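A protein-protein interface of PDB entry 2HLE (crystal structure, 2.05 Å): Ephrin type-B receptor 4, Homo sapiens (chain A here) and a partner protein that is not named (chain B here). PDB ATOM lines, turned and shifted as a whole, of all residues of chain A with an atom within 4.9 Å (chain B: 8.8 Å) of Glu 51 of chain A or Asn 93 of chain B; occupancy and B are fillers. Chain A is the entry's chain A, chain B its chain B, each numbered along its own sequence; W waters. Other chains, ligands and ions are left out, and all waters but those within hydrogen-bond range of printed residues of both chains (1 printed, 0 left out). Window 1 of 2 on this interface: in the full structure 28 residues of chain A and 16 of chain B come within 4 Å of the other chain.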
ATOM      1  N   GLN A  33     -12.470  -8.624  16.105  1.00  0.00           N
ATOM      2  CA  GLN A  33     -12.442  -7.527  17.017  1.00  0.00           C
ATOM      3  C   GLN A  33     -13.866  -7.118  17.397  1.00  0.00           C
ATOM      4  O   GLN A  33     -14.819  -7.491  16.738  1.00  0.00           O
ATOM      5  CB  GLN A  33     -11.684  -6.357  16.367  1.00  0.00           C
ATOM      6  CG  GLN A  33     -12.446  -5.674  15.176  1.00  0.00           C
ATOM      7  CD  GLN A  33     -11.687  -4.548  14.521  1.00  0.00           C
ATOM      8  OE1 GLN A  33     -11.121  -3.699  15.182  1.00  0.00           O
ATOM      9  NE2 GLN A  33     -11.685  -4.539  13.213  1.00  0.00           N
ATOM     10  N   TRP A  34     -14.007  -6.308  18.454  1.00  0.00           N
ATOM     11  CA  TRP A  34     -15.283  -5.805  18.816  1.00  0.00           C
ATOM     12  C   TRP A  34     -15.728  -4.885  17.710  1.00  0.00           C
ATOM     13  O   TRP A  34     -14.902  -4.266  17.064  1.00  0.00           O
ATOM     14  CB  TRP A  34     -15.231  -4.934  20.052  1.00  0.00           C
ATOM     15  CG  TRP A  34     -14.853  -5.570  21.326  1.00  0.00           C
ATOM     16  CD1 TRP A  34     -13.603  -5.925  21.744  1.00  0.00           C
ATOM     17  CD2 TRP A  34     -15.740  -5.887  22.395  1.00  0.00           C
ATOM     18  NE1 TRP A  34     -13.662  -6.456  23.026  1.00  0.00           N
ATOM     19  CE2 TRP A  34     -14.957  -6.405  23.455  1.00  0.00           C
ATOM     20  CE3 TRP A  34     -17.091  -5.738  22.581  1.00  0.00           C
ATOM     21  CZ2 TRP A  34     -15.499  -6.772  24.662  1.00  0.00           C
ATOM     22  CZ3 TRP A  34     -17.626  -6.069  23.806  1.00  0.00           C
ATOM     23  CH2 TRP A  34     -16.835  -6.589  24.818  1.00  0.00           C
ATOM     24  N   GLU A  35     -17.046  -4.714  17.621  1.00  0.00           N
ATOM     25  CA  GLU A  35     -17.668  -4.078  16.495  1.00  0.00           C
ATOM     26  C   GLU A  35     -18.849  -3.311  16.979  1.00  0.00           C
ATOM     27  O   GLU A  35     -19.671  -3.816  17.752  1.00  0.00           O
ATOM     28  CB  GLU A  35     -18.098  -5.175  15.522  1.00  0.00           C
ATOM     29  CG  GLU A  35     -18.873  -4.675  14.413  1.00  0.00           C
ATOM     30  CD  GLU A  35     -18.567  -5.398  13.211  1.00  0.00           C
ATOM     31  OE1 GLU A  35     -18.053  -4.727  12.301  1.00  0.00           O
ATOM     32  OE2 GLU A  35     -18.762  -6.641  13.201  1.00  0.00           O
ATOM     33  N   LEU A  37     -22.394  -1.280  16.233  1.00  0.00           N
ATOM     34  CA  LEU A  37     -23.605  -1.313  15.426  1.00  0.00           C
ATOM     35  C   LEU A  37     -24.808  -0.894  16.282  1.00  0.00           C
ATOM     36  O   LEU A  37     -24.732  -0.865  17.516  1.00  0.00           O
ATOM     37  CB  LEU A  37     -23.830  -2.729  14.773  1.00  0.00           C
ATOM     38  CG  LEU A  37     -23.640  -4.091  15.500  1.00  0.00           C
ATOM     39  CD1 LEU A  37     -23.188  -3.933  16.899  1.00  0.00           C
ATOM     40  CD2 LEU A  37     -24.945  -5.047  15.461  1.00  0.00           C
ATOM     41  N   GLY A  39     -28.531  -1.415  17.990  1.00  0.00           N
ATOM     42  CA  GLY A  39     -29.474  -2.408  18.370  1.00  0.00           C
ATOM     43  C   GLY A  39     -30.541  -1.868  19.288  1.00  0.00           C
ATOM     44  O   GLY A  39     -30.514  -0.735  19.696  1.00  0.00           O
ATOM     45  N   LEU A  40     -31.442  -2.752  19.657  1.00  0.00           N
ATOM     46  CA  LEU A  40     -32.502  -2.449  20.580  1.00  0.00           C
ATOM     47  C   LEU A  40     -32.061  -2.946  21.941  1.00  0.00           C
ATOM     48  O   LEU A  40     -31.255  -3.879  22.049  1.00  0.00           O
ATOM     49  CB  LEU A  40     -33.804  -3.120  20.094  1.00  0.00           C
ATOM     50  CG  LEU A  40     -34.834  -2.202  19.431  1.00  0.00           C
ATOM     51  CD1 LEU A  40     -34.262  -1.388  18.281  1.00  0.00           C
ATOM     52  CD2 LEU A  40     -36.050  -3.018  18.971  1.00  0.00           C
ATOM     53  N   THR A  49     -24.420  -0.099  20.176  1.00  0.00           N
ATOM     54  CA  THR A  49     -23.968  -1.280  20.942  1.00  0.00           C
ATOM     55  C   THR A  49     -22.553  -1.700  20.489  1.00  0.00           C
ATOM     56  O   THR A  49     -22.111  -1.249  19.404  1.00  0.00           O
ATOM     57  CB  THR A  49     -24.966  -2.437  20.792  1.00  0.00           C
ATOM     58  OG1 THR A  49     -24.950  -2.949  19.452  1.00  0.00           O
ATOM     59  CG2 THR A  49     -26.402  -1.975  21.214  1.00  0.00           C
ATOM     60  N   TYR A  50     -21.862  -2.505  21.311  1.00  0.00           N
ATOM     61  CA  TYR A  50     -20.580  -3.179  20.895  1.00  0.00           C
ATOM     62  C   TYR A  50     -20.729  -4.690  21.030  1.00  0.00           C
ATOM     63  O   TYR A  50     -21.229  -5.217  22.028  1.00  0.00           O
ATOM     64  CB  TYR A  50     -19.356  -2.710  21.665  1.00  0.00           C
ATOM     65  CG  TYR A  50     -18.636  -1.542  20.993  1.00  0.00           C
ATOM     66  CD1 TYR A  50     -17.792  -1.752  19.912  1.00  0.00           C
ATOM     67  CD2 TYR A  50     -18.878  -0.237  21.393  1.00  0.00           C
ATOM     68  CE1 TYR A  50     -17.197  -0.695  19.256  1.00  0.00           C
ATOM     69  CE2 TYR A  50     -18.316   0.824  20.724  1.00  0.00           C
ATOM     70  CZ  TYR A  50     -17.458   0.601  19.693  1.00  0.00           C
ATOM     71  OH  TYR A  50     -16.853   1.685  19.056  1.00  0.00           O
ATOM     72  N   GLU A  51     -20.311  -5.416  20.054  1.00  0.00           N
ATOM     73  CA  GLU A  51     -20.384  -6.885  20.147  1.00  0.00           C
ATOM     74  C   GLU A  51     -19.024  -7.499  19.961  1.00  0.00           C
ATOM     75  O   GLU A  51     -18.211  -7.007  19.171  1.00  0.00           O
ATOM     76  CB  GLU A  51     -21.294  -7.434  19.067  1.00  0.00           C
ATOM     77  CG  GLU A  51     -22.750  -7.071  19.314  1.00  0.00           C
ATOM     78  CD  GLU A  51     -23.684  -7.564  18.231  1.00  0.00           C
ATOM     79  OE1 GLU A  51     -23.194  -8.141  17.252  1.00  0.00           O
ATOM     80  OE2 GLU A  51     -24.915  -7.368  18.356  1.00  0.00           O
ATOM     81  N   VAL A  52     -18.781  -8.599  20.663  1.00  0.00           N
ATOM     82  CA  VAL A  52     -17.691  -9.485  20.267  1.00  0.00           C
ATOM     83  C   VAL A  52     -18.222 -10.933  20.300  1.00  0.00           C
ATOM     84  O   VAL A  52     -19.043 -11.283  21.143  1.00  0.00           O
ATOM     85  CB  VAL A  52     -16.472  -9.207  21.130  1.00  0.00           C
ATOM     86  CG1 VAL A  52     -16.793  -9.597  22.537  1.00  0.00           C
ATOM     87  CG2 VAL A  52     -15.190  -9.920  20.558  1.00  0.00           C
ATOM     88  N   CYS A  53     -17.848 -11.761  19.333  1.00  0.00           N
ATOM     89  CA  CYS A  53     -18.134 -13.204  19.449  1.00  0.00           C
ATOM     90  C   CYS A  53     -17.187 -14.085  18.601  1.00  0.00           C
ATOM     91  O   CYS A  53     -17.584 -14.678  17.606  1.00  0.00           O
ATOM     92  CB  CYS A  53     -19.620 -13.462  19.262  1.00  0.00           C
ATOM     93  SG  CYS A  53     -20.193 -15.178  19.333  1.00  0.00           S
ATOM     94  N   THR A  85     -25.566  -8.698  27.347  1.00  0.00           N
ATOM     95  CA  THR A  85     -26.107 -10.038  27.152  1.00  0.00           C
ATOM     96  C   THR A  85     -24.851 -10.907  26.903  1.00  0.00           C
ATOM     97  O   THR A  85     -23.796 -10.458  26.318  1.00  0.00           O
ATOM     98  CB  THR A  85     -27.189 -10.153  26.003  1.00  0.00           C
ATOM     99  OG1 THR A  85     -26.647  -9.692  24.781  1.00  0.00           O
ATOM    100  CG2 THR A  85     -28.412  -9.355  26.300  1.00  0.00           C
ATOM    101  N   LYS A 141     -29.704 -18.582  21.791  1.00  0.00           N
ATOM    102  CA  LYS A 141     -30.256 -18.109  20.529  1.00  0.00           C
ATOM    103  C   LYS A 141     -30.260 -19.207  19.499  1.00  0.00           C
ATOM    104  O   LYS A 141     -29.371 -20.035  19.473  1.00  0.00           O
ATOM    105  CB  LYS A 141     -29.353 -17.004  19.965  1.00  0.00           C
ATOM    106  CG  LYS A 141     -29.058 -15.923  20.951  1.00  0.00           C
ATOM    107  CD  LYS A 141     -28.785 -14.610  20.290  1.00  0.00           C
ATOM    108  CE  LYS A 141     -30.031 -13.949  19.738  1.00  0.00           C
ATOM    109  NZ  LYS A 141     -29.664 -12.818  18.858  1.00  0.00           N
ATOM    110  N   MET A 177     -20.687 -11.916  23.710  1.00  0.00           N
ATOM    111  CA  MET A 177     -21.389 -10.870  24.447  1.00  0.00           C
ATOM    112  C   MET A 177     -21.705  -9.600  23.651  1.00  0.00           C
ATOM    113  O   MET A 177     -20.979  -9.238  22.717  1.00  0.00           O
ATOM    114  CB  MET A 177     -20.639 -10.503  25.694  1.00  0.00           C
ATOM    115  CG  MET A 177     -19.254  -9.973  25.467  1.00  0.00           C
ATOM    116  SD  MET A 177     -18.565  -9.305  26.938  1.00  0.00           S
ATOM    117  CE  MET A 177     -19.761  -7.991  27.325  1.00  0.00           C
ATOM    118  N   ALA A 178     -22.861  -8.997  23.953  1.00  0.00           N
ATOM    119  CA  ALA A 178     -23.229  -7.700  23.423  1.00  0.00           C
ATOM    120  C   ALA A 178     -23.156  -6.731  24.620  1.00  0.00           C
ATOM    121  O   ALA A 178     -23.780  -6.974  25.636  1.00  0.00           O
ATOM    122  CB  ALA A 178     -24.695  -7.657  22.852  1.00  0.00           C
ATOM    123  N   LEU A 180     -24.669  -3.614  25.626  1.00  0.00           N
ATOM    124  CA  LEU A 180     -25.819  -2.831  25.208  1.00  0.00           C
ATOM    125  C   LEU A 180     -25.683  -1.364  25.629  1.00  0.00           C
ATOM    126  O   LEU A 180     -26.156  -0.486  24.910  1.00  0.00           O
ATOM    127  CB  LEU A 180     -27.123  -3.439  25.784  1.00  0.00           C
ATOM    128  CG  LEU A 180     -27.285  -4.938  25.548  1.00  0.00           C
ATOM    129  CD1 LEU A 180     -28.629  -5.387  25.936  1.00  0.00           C
ATOM    130  CD2 LEU A 180     -27.101  -5.301  24.098  1.00  0.00           C
ATOM    131  N   LYS B  30     -22.109  -3.050   6.431  1.00  0.00           N
ATOM    132  CA  LYS B  30     -22.719  -2.107   7.385  1.00  0.00           C
ATOM    133  C   LYS B  30     -23.439  -0.986   6.637  1.00  0.00           C
ATOM    134  O   LYS B  30     -22.940  -0.514   5.645  1.00  0.00           O
ATOM    135  CB  LYS B  30     -21.664  -1.450   8.281  1.00  0.00           C
ATOM    136  CG  LYS B  30     -21.222  -2.248   9.503  1.00  0.00           C
ATOM    137  CD  LYS B  30     -20.746  -1.233  10.591  1.00  0.00           C
ATOM    138  CE  LYS B  30     -19.831  -1.833  11.628  1.00  0.00           C
ATOM    139  NZ  LYS B  30     -19.576  -0.843  12.771  1.00  0.00           N
ATOM    140  N   PHE B  83     -29.613   4.769  12.327  1.00  0.00           N
ATOM    141  CA  PHE B  83     -29.501   3.363  12.720  1.00  0.00           C
ATOM    142  C   PHE B  83     -28.435   2.789  11.852  1.00  0.00           C
ATOM    143  O   PHE B  83     -28.444   3.020  10.625  1.00  0.00           O
ATOM    144  CB  PHE B  83     -30.818   2.549  12.522  1.00  0.00           C
ATOM    145  CG  PHE B  83     -30.803   1.156  13.214  1.00  0.00           C
ATOM    146  CD1 PHE B  83     -31.233   1.004  14.513  1.00  0.00           C
ATOM    147  CD2 PHE B  83     -30.334   0.034  12.538  1.00  0.00           C
ATOM    148  CE1 PHE B  83     -31.241  -0.234  15.112  1.00  0.00           C
ATOM    149  CE2 PHE B  83     -30.293  -1.178  13.111  1.00  0.00           C
ATOM    150  CZ  PHE B  83     -30.752  -1.340  14.417  1.00  0.00           C
ATOM    151  N   THR B  84     -27.478   2.083  12.442  1.00  0.00           N
ATOM    152  CA  THR B  84     -26.581   1.313  11.608  1.00  0.00           C
ATOM    153  C   THR B  84     -26.745  -0.192  11.791  1.00  0.00           C
ATOM    154  O   THR B  84     -26.557  -0.762  12.839  1.00  0.00           O
ATOM    155  CB  THR B  84     -25.116   1.743  11.572  1.00  0.00           C
ATOM    156  OG1 THR B  84     -24.224   0.627  11.735  1.00  0.00           O
ATOM    157  CG2 THR B  84     -24.827   2.943  12.426  1.00  0.00           C
ATOM    158  N   LYS B  86     -25.551  -3.820  10.934  1.00  0.00           N
ATOM    159  CA  LYS B  86     -24.544  -4.737  10.494  1.00  0.00           C
ATOM    160  C   LYS B  86     -25.257  -6.008   9.977  1.00  0.00           C
ATOM    161  O   LYS B  86     -26.015  -6.660  10.704  1.00  0.00           O
ATOM    162  CB  LYS B  86     -23.601  -5.094  11.651  1.00  0.00           C
ATOM    163  CG  LYS B  86     -22.746  -6.310  11.364  1.00  0.00           C
ATOM    164  CD  LYS B  86     -21.415  -5.912  10.848  1.00  0.00           C
ATOM    165  CE  LYS B  86     -20.479  -7.092  10.755  1.00  0.00           C
ATOM    166  NZ  LYS B  86     -19.172  -6.522  10.305  1.00  0.00           N
ATOM    167  N   GLN B  88     -25.098  -9.364   9.547  1.00  0.00           N
ATOM    168  CA  GLN B  88     -24.340 -10.475  10.102  1.00  0.00           C
ATOM    169  C   GLN B  88     -25.325 -11.621  10.366  1.00  0.00           C
ATOM    170  O   GLN B  88     -26.510 -11.371  10.616  1.00  0.00           O
ATOM    171  CB  GLN B  88     -23.637 -10.037  11.419  1.00  0.00           C
ATOM    172  CG  GLN B  88     -24.555  -9.468  12.473  1.00  0.00           C
ATOM    173  CD  GLN B  88     -23.867  -9.148  13.787  1.00  0.00           C
ATOM    174  OE1 GLN B  88     -22.862  -9.728  14.140  1.00  0.00           O
ATOM    175  NE2 GLN B  88     -24.396  -8.188  14.493  1.00  0.00           N
ATOM    176  N   GLU B  89     -24.834 -12.861  10.333  1.00  0.00           N
ATOM    177  CA  GLU B  89     -25.712 -14.072  10.437  1.00  0.00           C
ATOM    178  C   GLU B  89     -26.171 -14.364  11.888  1.00  0.00           C
ATOM    179  O   GLU B  89     -27.219 -14.946  12.135  1.00  0.00           O
ATOM    180  CB  GLU B  89     -25.024 -15.318   9.807  1.00  0.00           C
ATOM    181  CG  GLU B  89     -25.906 -16.137   8.813  1.00  0.00           C
ATOM    182  CD  GLU B  89     -25.789 -15.708   7.333  1.00  0.00           C
ATOM    183  OE1 GLU B  89     -25.302 -14.582   7.083  1.00  0.00           O
ATOM    184  OE2 GLU B  89     -26.197 -16.482   6.412  1.00  0.00           O
ATOM    185  N   PHE B  90     -25.410 -13.867  12.845  1.00  0.00           N
ATOM    186  CA  PHE B  90     -25.625 -14.146  14.262  1.00  0.00           C
ATOM    187  C   PHE B  90     -25.220 -12.901  15.039  1.00  0.00           C
ATOM    188  O   PHE B  90     -24.088 -12.406  14.862  1.00  0.00           O
ATOM    189  CB  PHE B  90     -24.726 -15.328  14.659  1.00  0.00           C
ATOM    190  CG  PHE B  90     -24.949 -15.836  16.043  1.00  0.00           C
ATOM    191  CD1 PHE B  90     -26.075 -16.569  16.338  1.00  0.00           C
ATOM    192  CD2 PHE B  90     -24.035 -15.572  17.052  1.00  0.00           C
ATOM    193  CE1 PHE B  90     -26.303 -17.038  17.631  1.00  0.00           C
ATOM    194  CE2 PHE B  90     -24.268 -16.018  18.347  1.00  0.00           C
ATOM    195  CZ  PHE B  90     -25.410 -16.778  18.625  1.00  0.00           C
ATOM    196  N   SER B  91     -26.121 -12.401  15.880  1.00  0.00           N
ATOM    197  CA  SER B  91     -25.794 -11.386  16.888  1.00  0.00           C
ATOM    198  C   SER B  91     -25.875 -11.867  18.344  1.00  0.00           C
ATOM    199  O   SER B  91     -26.864 -12.466  18.719  1.00  0.00           O
ATOM    200  CB  SER B  91     -26.729 -10.201  16.686  1.00  0.00           C
ATOM    201  OG  SER B  91     -26.708  -9.303  17.776  1.00  0.00           O
ATOM    202  N   PRO B  92     -24.833 -11.573  19.200  1.00  0.00           N
ATOM    203  CA  PRO B  92     -24.937 -11.809  20.654  1.00  0.00           C
ATOM    204  C   PRO B  92     -25.910 -10.942  21.467  1.00  0.00           C
ATOM    205  O   PRO B  92     -26.114 -11.229  22.657  1.00  0.00           O
ATOM    206  CB  PRO B  92     -23.524 -11.609  21.147  1.00  0.00           C
ATOM    207  CG  PRO B  92     -22.840 -10.754  20.134  1.00  0.00           C
ATOM    208  CD  PRO B  92     -23.450 -11.175  18.843  1.00  0.00           C
ATOM    209  N   ASN B  93     -26.473  -9.918  20.819  1.00  0.00           N
ATOM    210  CA  ASN B  93     -27.639  -9.201  21.296  1.00  0.00           C
ATOM    211  C   ASN B  93     -28.922 -10.042  21.186  1.00  0.00           C
ATOM    212  O   ASN B  93     -29.327 -10.532  20.116  1.00  0.00           O
ATOM    213  CB  ASN B  93     -27.831  -7.888  20.529  1.00  0.00           C
ATOM    214  CG  ASN B  93     -28.829  -6.913  21.214  1.00  0.00           C
ATOM    215  OD1 ASN B  93     -29.525  -7.281  22.138  1.00  0.00           O
ATOM    216  ND2 ASN B  93     -28.830  -5.621  20.762  1.00  0.00           N
ATOM    217  N   LEU B  94     -29.548 -10.178  22.326  1.00  0.00           N
ATOM    218  CA  LEU B  94     -30.832 -10.810  22.470  1.00  0.00           C
ATOM    219  C   LEU B  94     -31.845 -10.235  21.453  1.00  0.00           C
ATOM    220  O   LEU B  94     -32.632 -10.967  20.897  1.00  0.00           O
ATOM    221  CB  LEU B  94     -31.272 -10.639  23.942  1.00  0.00           C
ATOM    222  CG  LEU B  94     -32.669 -11.091  24.388  1.00  0.00           C
ATOM    223  CD1 LEU B  94     -32.741 -12.581  24.280  1.00  0.00           C
ATOM    224  CD2 LEU B  94     -32.816 -10.606  25.824  1.00  0.00           C
ATOM    225  N   TRP B  95     -31.775  -8.933  21.172  1.00  0.00           N
ATOM    226  CA  TRP B  95     -32.588  -8.285  20.126  1.00  0.00           C
ATOM    227  C   TRP B  95     -31.803  -7.900  18.903  1.00  0.00           C
ATOM    228  O   TRP B  95     -32.216  -7.051  18.146  1.00  0.00           O
ATOM    229  CB  TRP B  95     -33.210  -6.995  20.663  1.00  0.00           C
ATOM    230  CG  TRP B  95     -34.057  -7.244  21.821  1.00  0.00           C
ATOM    231  CD1 TRP B  95     -35.341  -7.704  21.820  1.00  0.00           C
ATOM    232  CD2 TRP B  95     -33.678  -7.092  23.183  1.00  0.00           C
ATOM    233  NE1 TRP B  95     -35.791  -7.850  23.112  1.00  0.00           N
ATOM    234  CE2 TRP B  95     -34.783  -7.480  23.970  1.00  0.00           C
ATOM    235  CE3 TRP B  95     -32.504  -6.655  23.822  1.00  0.00           C
ATOM    236  CZ2 TRP B  95     -34.759  -7.429  25.370  1.00  0.00           C
ATOM    237  CZ3 TRP B  95     -32.488  -6.614  25.217  1.00  0.00           C
ATOM    238  CH2 TRP B  95     -33.601  -7.009  25.969  1.00  0.00           C
ATOM    239  N   GLY B  96     -30.662  -8.503  18.684  1.00  0.00           N
ATOM    240  CA  GLY B  96     -29.872  -8.157  17.499  1.00  0.00           C
ATOM    241  C   GLY B  96     -30.505  -8.539  16.174  1.00  0.00           C
ATOM    242  O   GLY B  96     -31.306  -9.489  16.108  1.00  0.00           O
ATOM    243  N   LEU B  97     -30.124  -7.820  15.107  1.00  0.00           N
ATOM    244  CA  LEU B  97     -30.635  -8.094  13.777  1.00  0.00           C
ATOM    245  C   LEU B  97     -29.729  -9.170  13.145  1.00  0.00           C
ATOM    246  O   LEU B  97     -28.492  -9.087  13.201  1.00  0.00           O
ATOM    247  CB  LEU B  97     -30.691  -6.812  12.906  1.00  0.00           C
ATOM    248  CG  LEU B  97     -31.687  -5.655  13.168  1.00  0.00           C
ATOM    249  CD1 LEU B  97     -31.468  -4.455  12.229  1.00  0.00           C
ATOM    250  CD2 LEU B  97     -33.120  -6.042  13.075  1.00  0.00           C
ATOM    251  N   GLU B  98     -30.356 -10.184  12.551  1.00  0.00           N
ATOM    252  CA  GLU B  98     -29.674 -11.414  12.085  1.00  0.00           C
ATOM    253  C   GLU B  98     -30.138 -11.763  10.662  1.00  0.00           C
ATOM    254  O   GLU B  98     -31.341 -11.777  10.439  1.00  0.00           O
ATOM    255  CB  GLU B  98     -30.011 -12.562  13.056  1.00  0.00           C
ATOM    256  CG  GLU B  98     -29.649 -12.258  14.513  1.00  0.00           C
ATOM    257  CD  GLU B  98     -29.674 -13.484  15.437  1.00  0.00           C
ATOM    258  OE1 GLU B  98     -30.460 -14.433  15.192  1.00  0.00           O
ATOM    259  OE2 GLU B  98     -28.890 -13.495  16.436  1.00  0.00           O
HETATM  260  O   HOH W   1     -26.397  -5.168  19.114  1.00  0.00           O
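NZ of Lys 86 of chain B lies within salt-bridge range of OE1 of Glu 35 of chain A, at 2.9 Å. O of Leu 40 of chain A lies within hydrogen-bond range of ND2 of Asn 93 of chain B (3.3 Å). OE1 of Glu 51 of chain A sits at hydrogen-bond distance from NE2 of Gln 88 of chain B. The side-chain carboxylate (OE2) of Glu 51 of chain A is in hydrogen-bond range of the side-chain hydroxyl (OG) of Ser 91 of chain B, 2.7 Å away. The backbone carbonyl oxygen (O) of Pro 92 of chain B sits at hydrogen-bond distance from the side-chain hydroxyl (OG1) of Thr 85 of chain A, at 2.7 Å. O of Ser 91 of chain B is in hydrogen-bond range of NZ of Lys 141 of chain A (2.8 Å). O of Asn 93 of chain B is in hydrogen-bond range of NZ of Lys 141 of chain A, 2.6 Å away. The side-chain amino group (NZ) of Lys 141 of chain A lies within salt-bridge range of the side-chain carboxylate (OE2) of Glu 98 of chain B, at 2.6 Å.
O of Glu 35 of chain A is in hydrogen-bond range of N of Glu 51 of chain A. The backbone carbonyl oxygen (O) of Leu 37 of chain A lies within hydrogen-bond range of the backbone NH (N) of Thr 49 of chain A, at 2.8 Å. N of Ala 178 of chain A is in hydrogen-bond range of O of Thr 85 of chain A (2.9 Å). The side-chain hydroxyl (OG) of Ser 91 of chain B sits at hydrogen-bond distance from the backbone NH (N) of Asn 93 of chain B, at 3.1 Å. N of Ser 91 of chain B lies within hydrogen-bond range of OE2 of Glu 98 of chain B, at 3.0 Å. The backbone NH of Trp 95 of chain B sits at hydrogen-bond distance from the side-chain amide oxygen of Asn 93 of chain B, at 3.0 Å.
Among the printed residues, merely in contact across the chains: Glu 35 of chain A with Lys 30 of chain B (3.5 Å), Leu 37 of chain A with Thr 84 of chain B (3.9 Å), Leu 37 of chain A with Lys 86 of chain B (3.9 Å), Leu 37 of chain A with Gln 88 of chain B (3.3 Å), Leu 40 of chain A with Trp 95 of chain B (3.5 Å), Glu 51 of chain A with Pro 92 of chain B (3.4 Å), Glu 51 of chain A with Asn 93 of chain B (3.7 Å), Val 52 of chain A with Pro 92 of chain B (3.96 Å), Thr 85 of chain A with Asn 93 of chain B (3.7 Å), Thr 85 of chain A with Leu 94 of chain B (3.8 Å), Lys 141 of chain A with Phe 90 of chain B (3.8 Å), Met 177 of chain A with Pro 92 of chain B (3.5 Å), Ala 178 of chain A with Pro 92 of chain B (3.8 Å), Ala 178 of chain A with Asn 93 of chain B (3.5 Å) and Leu 180 of chain A with Asn 93 of chain B (3.7 Å).
Printed residues of chain B within 4 Å of Glu 51 of chain A: Gln 88 (3.0 Å), Ser 91 (2.7 Å), Pro 92 (3.4 Å) and Asn 93 (3.7 Å). Printed residues of chain B within 4 Å of Thr 85 of chain A: Pro 92, Asn 93 and Leu 94. Printed residues of chain B within 4 Å of Ala 178 of chain A: Pro 92 and Asn 93. Asn 93 of chain B touches six residues of chain A. The nearest printed residue of chain A that does not touch Phe 90 of chain B is Cys 53 of chain A (4.3 Å).
Of the 16 printed residues of chain A, 10 touch a printed residue of chain B. Hydrophobic or aromatic side chains of chain B that line the printed part of chain A: Phe 90, Pro 92, Leu 94 and Trp 95. Among the printed residues, Asp or Glu carboxylates within 4 Å of a Lys or Arg side-chain nitrogen of the other chain: Glu 35 of chain A with Lys 86 of chain B and Lys 141 of chain A with Glu 98 of chain B.
Water W1 lies within hydrogen-bond range of the side-chain hydroxyl of Thr 49 of chain A (2.7 Å), the side-chain carboxylate of Glu 51 of chain A (2.8 Å) and the side-chain amide nitrogen of Asn 93 of chain B (3.0 Å).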
